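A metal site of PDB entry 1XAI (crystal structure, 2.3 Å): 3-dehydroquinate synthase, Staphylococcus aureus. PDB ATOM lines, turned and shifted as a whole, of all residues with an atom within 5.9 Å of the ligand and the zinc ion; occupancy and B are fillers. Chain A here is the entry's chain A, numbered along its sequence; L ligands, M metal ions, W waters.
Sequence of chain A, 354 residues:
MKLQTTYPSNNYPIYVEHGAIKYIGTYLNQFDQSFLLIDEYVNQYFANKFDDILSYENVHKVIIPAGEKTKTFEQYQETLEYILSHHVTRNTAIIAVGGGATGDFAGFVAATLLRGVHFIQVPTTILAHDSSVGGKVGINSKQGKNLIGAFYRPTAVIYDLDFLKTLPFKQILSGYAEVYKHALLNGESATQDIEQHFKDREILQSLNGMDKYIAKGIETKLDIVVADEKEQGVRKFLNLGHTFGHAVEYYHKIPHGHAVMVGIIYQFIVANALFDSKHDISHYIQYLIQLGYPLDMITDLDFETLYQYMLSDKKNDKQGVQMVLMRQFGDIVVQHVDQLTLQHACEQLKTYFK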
ATOM      1  N   ASP A 130      35.458  21.327 -13.813  1.00  0.00           N
ATOM      2  CA  ASP A 130      34.200  20.933 -13.221  1.00  0.00           C
ATOM      3  C   ASP A 130      34.161  21.298 -11.732  1.00  0.00           C
ATOM      4  O   ASP A 130      33.391  22.181 -11.339  1.00  0.00           O
ATOM      5  CB  ASP A 130      34.024  19.421 -13.380  1.00  0.00           C
ATOM      6  CG  ASP A 130      32.909  18.884 -12.543  1.00  0.00           C
ATOM      7  OD1 ASP A 130      31.818  19.478 -12.555  1.00  0.00           O
ATOM      8  OD2 ASP A 130      33.126  17.848 -11.864  1.00  0.00           O
ATOM      9  N   SER A 131      34.995  20.650 -10.927  1.00  0.00           N
ATOM     10  CA  SER A 131      35.038  20.902  -9.494  1.00  0.00           C
ATOM     11  C   SER A 131      35.230  22.357  -9.022  1.00  0.00           C
ATOM     12  O   SER A 131      34.808  22.708  -7.917  1.00  0.00           O
ATOM     13  CB  SER A 131      36.118  20.038  -8.837  1.00  0.00           C
ATOM     14  OG  SER A 131      37.414  20.371  -9.294  1.00  0.00           O
ATOM     15  N   VAL A 133      33.800  25.042 -10.230  1.00  0.00           N
ATOM     16  CA  VAL A 133      32.642  25.882 -10.440  1.00  0.00           C
ATOM     17  C   VAL A 133      31.412  25.275  -9.734  1.00  0.00           C
ATOM     18  O   VAL A 133      31.225  24.060  -9.722  1.00  0.00           O
ATOM     19  CB  VAL A 133      32.370  26.031 -11.962  1.00  0.00           C
ATOM     20  CG1 VAL A 133      31.410  27.188 -12.229  1.00  0.00           C
ATOM     21  CG2 VAL A 133      33.690  26.245 -12.698  1.00  0.00           C
ATOM     22  N   GLY A 134      30.597  26.130  -9.131  1.00  0.00           N
ATOM     23  CA  GLY A 134      29.406  25.647  -8.462  1.00  0.00           C
ATOM     24  C   GLY A 134      29.397  25.845  -6.960  1.00  0.00           C
ATOM     25  O   GLY A 134      28.335  25.842  -6.328  1.00  0.00           O
ATOM     26  N   LYS A 136      30.543  23.732  -4.617  1.00  0.00           N
ATOM     27  CA  LYS A 136      30.529  22.531  -3.765  1.00  0.00           C
ATOM     28  C   LYS A 136      31.927  22.178  -3.232  1.00  0.00           C
ATOM     29  O   LYS A 136      32.841  21.864  -4.001  1.00  0.00           O
ATOM     30  CB  LYS A 136      29.985  21.321  -4.524  1.00  0.00           C
ATOM     31  CG  LYS A 136      28.479  21.168  -4.474  1.00  0.00           C
ATOM     32  CD  LYS A 136      28.035  19.826  -5.062  1.00  0.00           C
ATOM     33  CE  LYS A 136      26.532  19.756  -5.215  1.00  0.00           C
ATOM     34  NZ  LYS A 136      26.066  18.500  -5.870  1.00  0.00           N
ATOM     35  N   LYS A 145      32.510   9.488  -0.336  1.00  0.00           N
ATOM     36  CA  LYS A 145      33.065  10.731  -0.850  1.00  0.00           C
ATOM     37  C   LYS A 145      32.123  11.908  -0.637  1.00  0.00           C
ATOM     38  O   LYS A 145      30.911  11.767  -0.741  1.00  0.00           O
ATOM     39  CB  LYS A 145      33.377  10.563  -2.353  1.00  0.00           C
ATOM     40  CG  LYS A 145      33.973  11.786  -3.031  1.00  0.00           C
ATOM     41  CD  LYS A 145      34.385  11.442  -4.461  1.00  0.00           C
ATOM     42  CE  LYS A 145      34.725  12.675  -5.294  1.00  0.00           C
ATOM     43  NZ  LYS A 145      35.986  13.358  -4.934  1.00  0.00           N
ATOM     44  N   ASN A 146      32.701  13.056  -0.303  1.00  0.00           N
ATOM     45  CA  ASN A 146      31.942  14.307  -0.098  1.00  0.00           C
ATOM     46  C   ASN A 146      30.715  14.243   0.809  1.00  0.00           C
ATOM     47  O   ASN A 146      29.638  14.744   0.432  1.00  0.00           O
ATOM     48  CB  ASN A 146      31.494  14.864  -1.449  1.00  0.00           C
ATOM     49  CG  ASN A 146      32.601  14.858  -2.466  1.00  0.00           C
ATOM     50  OD1 ASN A 146      33.787  14.784  -2.109  1.00  0.00           O
ATOM     51  ND2 ASN A 146      32.232  14.953  -3.744  1.00  0.00           N
ATOM     52  N   GLU A 178      34.569  14.284 -17.355  1.00  0.00           N
ATOM     53  CA  GLU A 178      33.642  15.369 -16.989  1.00  0.00           C
ATOM     54  C   GLU A 178      33.346  16.201 -18.229  1.00  0.00           C
ATOM     55  O   GLU A 178      32.211  16.663 -18.395  1.00  0.00           O
ATOM     56  CB  GLU A 178      34.234  16.274 -15.907  1.00  0.00           C
ATOM     57  CG  GLU A 178      34.530  15.617 -14.563  1.00  0.00           C
ATOM     58  CD  GLU A 178      33.304  15.162 -13.829  1.00  0.00           C
ATOM     59  OE1 GLU A 178      33.452  14.474 -12.799  1.00  0.00           O
ATOM     60  OE2 GLU A 178      32.187  15.495 -14.266  1.00  0.00           O
ATOM     61  N   LYS A 181      30.881  14.189 -19.993  1.00  0.00           N
ATOM     62  CA  LYS A 181      29.599  14.160 -19.289  1.00  0.00           C
ATOM     63  C   LYS A 181      28.748  15.379 -19.616  1.00  0.00           C
ATOM     64  O   LYS A 181      27.546  15.275 -19.829  1.00  0.00           O
ATOM     65  CB  LYS A 181      29.824  14.095 -17.776  1.00  0.00           C
ATOM     66  CG  LYS A 181      28.543  13.838 -16.969  1.00  0.00           C
ATOM     67  CD  LYS A 181      28.680  14.265 -15.508  1.00  0.00           C
ATOM     68  CE  LYS A 181      29.156  15.714 -15.373  1.00  0.00           C
ATOM     69  NZ  LYS A 181      29.314  16.172 -13.958  1.00  0.00           N
ATOM     70  N   LYS A 221      28.007  24.108 -17.066  1.00  0.00           N
ATOM     71  CA  LYS A 221      27.766  23.949 -15.645  1.00  0.00           C
ATOM     72  C   LYS A 221      27.279  25.251 -15.042  1.00  0.00           C
ATOM     73  O   LYS A 221      26.309  25.275 -14.290  1.00  0.00           O
ATOM     74  CB  LYS A 221      29.040  23.508 -14.907  1.00  0.00           C
ATOM     75  CG  LYS A 221      28.767  22.981 -13.488  1.00  0.00           C
ATOM     76  CD  LYS A 221      30.060  22.612 -12.755  1.00  0.00           C
ATOM     77  CE  LYS A 221      29.747  21.956 -11.434  1.00  0.00           C
ATOM     78  NZ  LYS A 221      30.953  21.628 -10.654  1.00  0.00           N
ATOM     79  N   VAL A 225      24.308  25.415 -12.262  1.00  0.00           N
ATOM     80  CA  VAL A 225      24.581  25.845 -10.896  1.00  0.00           C
ATOM     81  C   VAL A 225      23.933  27.186 -10.575  1.00  0.00           C
ATOM     82  O   VAL A 225      23.494  27.404  -9.442  1.00  0.00           O
ATOM     83  CB  VAL A 225      26.110  25.905 -10.589  1.00  0.00           C
ATOM     84  CG1 VAL A 225      26.753  24.564 -10.888  1.00  0.00           C
ATOM     85  CG2 VAL A 225      26.777  27.010 -11.387  1.00  0.00           C
ATOM     86  N   GLU A 231      21.198  22.468  -5.611  1.00  0.00           N
ATOM     87  CA  GLU A 231      20.839  21.159  -6.165  1.00  0.00           C
ATOM     88  C   GLU A 231      19.419  20.829  -5.736  1.00  0.00           C
ATOM     89  O   GLU A 231      19.167  19.790  -5.117  1.00  0.00           O
ATOM     90  CB  GLU A 231      21.794  20.050  -5.687  1.00  0.00           C
ATOM     91  CG  GLU A 231      21.691  18.725  -6.484  1.00  0.00           C
ATOM     92  CD  GLU A 231      22.431  17.533  -5.853  1.00  0.00           C
ATOM     93  OE1 GLU A 231      23.566  17.720  -5.348  1.00  0.00           O
ATOM     94  OE2 GLU A 231      21.888  16.402  -5.863  1.00  0.00           O
ATOM     95  N   ARG A 235      20.225  20.557 -10.870  1.00  0.00           N
ATOM     96  CA  ARG A 235      21.670  20.368 -10.681  1.00  0.00           C
ATOM     97  C   ARG A 235      21.985  18.907 -10.385  1.00  0.00           C
ATOM     98  O   ARG A 235      23.140  18.493 -10.357  1.00  0.00           O
ATOM     99  CB  ARG A 235      22.213  21.250  -9.538  1.00  0.00           C
ATOM    100  CG  ARG A 235      23.725  21.190  -9.387  1.00  0.00           C
ATOM    101  CD  ARG A 235      24.294  22.220  -8.395  1.00  0.00           C
ATOM    102  NE  ARG A 235      25.743  22.069  -8.293  1.00  0.00           N
ATOM    103  CZ  ARG A 235      26.597  22.928  -7.730  1.00  0.00           C
ATOM    104  NH1 ARG A 235      26.185  24.067  -7.167  1.00  0.00           N
ATOM    105  NH2 ARG A 235      27.895  22.652  -7.753  1.00  0.00           N
ATOM    106  N   LEU A 238      24.235  17.013 -12.950  1.00  0.00           N
ATOM    107  CA  LEU A 238      25.692  17.017 -13.055  1.00  0.00           C
ATOM    108  C   LEU A 238      26.196  15.725 -12.410  1.00  0.00           C
ATOM    109  O   LEU A 238      27.363  15.357 -12.528  1.00  0.00           O
ATOM    110  CB  LEU A 238      26.268  18.230 -12.334  1.00  0.00           C
ATOM    111  CG  LEU A 238      25.755  19.610 -12.754  1.00  0.00           C
ATOM    112  CD1 LEU A 238      26.607  20.694 -12.110  1.00  0.00           C
ATOM    113  CD2 LEU A 238      25.829  19.734 -14.269  1.00  0.00           C
ATOM    114  N   ASN A 239      25.276  15.025 -11.735  1.00  0.00           N
ATOM    115  CA  ASN A 239      25.536  13.763 -11.062  1.00  0.00           C
ATOM    116  C   ASN A 239      25.376  12.576 -12.003  1.00  0.00           C
ATOM    117  O   ASN A 239      25.297  11.422 -11.561  1.00  0.00           O
ATOM    118  CB  ASN A 239      24.570  13.601  -9.883  1.00  0.00           C
ATOM    119  CG  ASN A 239      25.236  13.789  -8.539  1.00  0.00           C
ATOM    120  OD1 ASN A 239      26.006  12.938  -8.096  1.00  0.00           O
ATOM    121  ND2 ASN A 239      24.947  14.917  -7.884  1.00  0.00           N
ATOM    122  N   HIS A 242      27.383   9.295 -11.465  1.00  0.00           N
ATOM    123  CA  HIS A 242      28.168   9.383 -10.238  1.00  0.00           C
ATOM    124  C   HIS A 242      27.634   8.478  -9.138  1.00  0.00           C
ATOM    125  O   HIS A 242      28.332   8.212  -8.158  1.00  0.00           O
ATOM    126  CB  HIS A 242      28.204  10.811  -9.704  1.00  0.00           C
ATOM    127  CG  HIS A 242      29.019  11.743 -10.532  1.00  0.00           C
ATOM    128  ND1 HIS A 242      28.820  11.918 -11.882  1.00  0.00           N
ATOM    129  CD2 HIS A 242      30.022  12.594 -10.184  1.00  0.00           C
ATOM    130  CE1 HIS A 242      29.658  12.828 -12.335  1.00  0.00           C
ATOM    131  NE2 HIS A 242      30.398  13.255 -11.333  1.00  0.00           N
ATOM    132  N   HIS A 246      30.717   7.050  -7.865  1.00  0.00           N
ATOM    133  CA  HIS A 246      31.256   7.382  -6.554  1.00  0.00           C
ATOM    134  C   HIS A 246      31.524   6.137  -5.726  1.00  0.00           C
ATOM    135  O   HIS A 246      32.423   6.124  -4.884  1.00  0.00           O
ATOM    136  CB  HIS A 246      30.313   8.308  -5.804  1.00  0.00           C
ATOM    137  CG  HIS A 246      30.522   9.756  -6.098  1.00  0.00           C
ATOM    138  ND1 HIS A 246      29.584  10.725  -5.804  1.00  0.00           N
ATOM    139  CD2 HIS A 246      31.579  10.409  -6.631  1.00  0.00           C
ATOM    140  CE1 HIS A 246      30.058  11.915  -6.140  1.00  0.00           C
ATOM    141  NE2 HIS A 246      31.265  11.750  -6.645  1.00  0.00           N
ATOM    142  N   HIS A 256      38.722   9.701 -10.400  1.00  0.00           N
ATOM    143  CA  HIS A 256      37.343  10.143 -10.500  1.00  0.00           C
ATOM    144  C   HIS A 256      36.715   9.969 -11.876  1.00  0.00           C
ATOM    145  O   HIS A 256      35.648   9.372 -11.983  1.00  0.00           O
ATOM    146  CB  HIS A 256      37.216  11.606 -10.077  1.00  0.00           C
ATOM    147  CG  HIS A 256      35.804  12.036  -9.876  1.00  0.00           C
ATOM    148  ND1 HIS A 256      34.893  11.289  -9.156  1.00  0.00           N
ATOM    149  CD2 HIS A 256      35.126  13.110 -10.342  1.00  0.00           C
ATOM    150  CE1 HIS A 256      33.721  11.892  -9.184  1.00  0.00           C
ATOM    151  NE2 HIS A 256      33.836  13.000  -9.889  1.00  0.00           N
ATOM    152  N   VAL A 260      33.684   7.647 -13.212  1.00  0.00           N
ATOM    153  CA  VAL A 260      32.534   8.300 -13.840  1.00  0.00           C
ATOM    154  C   VAL A 260      32.196   7.650 -15.199  1.00  0.00           C
ATOM    155  O   VAL A 260      31.030   7.347 -15.462  1.00  0.00           O
ATOM    156  CB  VAL A 260      32.754   9.836 -14.011  1.00  0.00           C
ATOM    157  CG1 VAL A 260      31.746  10.404 -15.000  1.00  0.00           C
ATOM    158  CG2 VAL A 260      32.583  10.541 -12.678  1.00  0.00           C
ATOM    159  N   LYS A 314      24.079  11.072  -1.758  1.00  0.00           N
ATOM    160  CA  LYS A 314      23.393  12.298  -1.387  1.00  0.00           C
ATOM    161  C   LYS A 314      22.131  12.609  -2.176  1.00  0.00           C
ATOM    162  O   LYS A 314      21.476  13.622  -1.939  1.00  0.00           O
ATOM    163  CB  LYS A 314      24.362  13.490  -1.493  1.00  0.00           C
ATOM    164  CG  LYS A 314      25.427  13.549  -0.410  1.00  0.00           C
ATOM    165  CD  LYS A 314      26.257  14.834  -0.497  1.00  0.00           C
ATOM    166  CE  LYS A 314      27.179  14.827  -1.700  1.00  0.00           C
ATOM    167  NZ  LYS A 314      28.197  13.732  -1.603  1.00  0.00           N
HETATM  168  C1  LIG L   1      28.089  19.432  -8.964  1.00  0.00           C
HETATM  169  O1  LIG L   1      26.821  19.585  -8.830  1.00  0.00           O
HETATM  170  O2  LIG L   1      28.929  20.360  -8.949  1.00  0.00           O
HETATM  171  C2  LIG L   1      28.541  17.971  -9.131  1.00  0.00           C
HETATM  172  O3  LIG L   1      27.405  17.130  -9.329  1.00  0.00           O
HETATM  173  C3  LIG L   1      29.515  17.740 -10.306  1.00  0.00           C
HETATM  174  C4  LIG L   1      30.229  16.383 -10.226  1.00  0.00           C
HETATM  175  O4  LIG L   1      31.284  16.291 -11.214  1.00  0.00           O
HETATM  176  C5  LIG L   1      30.843  16.144  -8.787  1.00  0.00           C
HETATM  177  O5  LIG L   1      31.428  14.880  -8.746  1.00  0.00           O
HETATM  178  C6  LIG L   1      29.715  16.280  -7.740  1.00  0.00           C
HETATM  179  C7  LIG L   1      30.089  15.959  -6.302  1.00  0.00           C
HETATM  180  C8  LIG L   1      29.202  17.655  -7.763  1.00  0.00           C
HETATM  181  P1  LIG L   1      28.783  15.254  -5.246  1.00  0.00           P
HETATM  182  O6  LIG L   1      28.042  14.230  -6.029  1.00  0.00           O
HETATM  183  O7  LIG L   1      27.958  16.482  -4.901  1.00  0.00           O
HETATM  184  O8  LIG L   1      29.603  14.660  -4.038  1.00  0.00           O
HETATM  185 ZN    ZN M   1      32.326  14.288 -10.913  1.00  0.00          ZN
HETATM  186  O   HOH W   1      30.971  22.654  -7.610  1.00  0.00           O
HETATM  187  O   HOH W   2      29.332  18.811 -13.614  1.00  0.00           O
HETATM  188  O   HOH W   3      34.937  16.258  -9.980  1.00  0.00           O
HETATM  189  O   HOH W   4      25.019  14.640  -4.811  1.00  0.00           O
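OD2 of Asp 130 lies close to O4 of the ligand (2.5 Å).
An oxygen (O8) of the ligand is in hydrogen-bond range of the side-chain amide nitrogen (ND2) of Asn 146.
The guanidinium group of Arg 235 is in salt-bridge range of an oxygen (O1) of the ligand (2.8 Å).
The side-chain amino group (NZ) of Lys 136 is in salt-bridge range of an oxygen (O7) of the ligand.
The side-chain amino group (NZ) of Lys 221 lies within salt-bridge range of an oxygen (O2) of the ligand.
NZ of Lys 314 lies within salt-bridge range of O8 of the ligand (3.0 Å).
The side-chain amide oxygen (OD1) of Asn 239 sits close to an oxygen (O6) of the ligand.
The side-chain amino group of Lys 181 lies close to an oxygen (O4) of the ligand (3.4 Å).
Residues that only touch the zinc ion: Asp 130 (3.8 Å).
Within 4 Å of the zinc ion: Asp 130, Glu 178, His 242 and His 256.
The nearest printed residue that does not touch the zinc ion is Val 260 (4.1 Å).
The side-chain amino group (NZ) of Lys 181 lies within salt-bridge range of the side-chain carboxylate (OE2) of Glu 178 (3.0 Å).
OD1 of Asp 130 lies within salt-bridge range of NZ of Lys 221 (3.0 Å).
O of Asn 146 is in hydrogen-bond range of NZ of Lys 314 (2.7 Å).
The backbone carbonyl oxygen of Gly 134 is in hydrogen-bond range of the guanidinium group of Arg 235 (2.9 Å).
The side-chain amino group (NZ) of Lys 136 lies within salt-bridge range of the side-chain carboxylate (OE1) of Glu 231 (2.7 Å).
The backbone carbonyl oxygen (O) of Val 133 lies within hydrogen-bond range of the side-chain amino group (NZ) of Lys 221 (2.6 Å).
O of Lys 145 is in hydrogen-bond range of NZ of Lys 314, at 3.5 Å.
NZ of Lys 181 lies within hydrogen-bond range of O of Leu 238 (2.6 Å).
The zinc ion is bound by the side-chain carboxylate (OE1) of Glu 178.
A ring nitrogen (NE2) of His 242 binds the zinc ion.
A ring nitrogen (NE2) of His 256 is bound to the zinc ion (2.2 Å).
The zinc ion is bound by an oxygen (O4) of the ligand (2.3 Å).
O5 of the ligand is bound to the zinc ion, 2.4 Å away.
Leu 238 touches the ligand.
CE1 of His 246 touches O6 of the ligand, 3.1 Å away.
Hydrophobic or aromatic side chains that line the ligand: Leu 238, His 242, His 246 and His 256.
The nearest printed residue that does not touch the ligand is Val 133 (4.4 Å).
Water W4 lies within hydrogen-bond range of the side-chain amide nitrogen of Asn 239 (3.1 Å), an oxygen (O6) of the ligand (3.3 Å) and the side-chain carboxylate of Glu 231 (3.4 Å).
Water W2 lies within hydrogen-bond range of the side-chain amino group of Lys 181 and the side-chain carboxylate of Asp 130.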
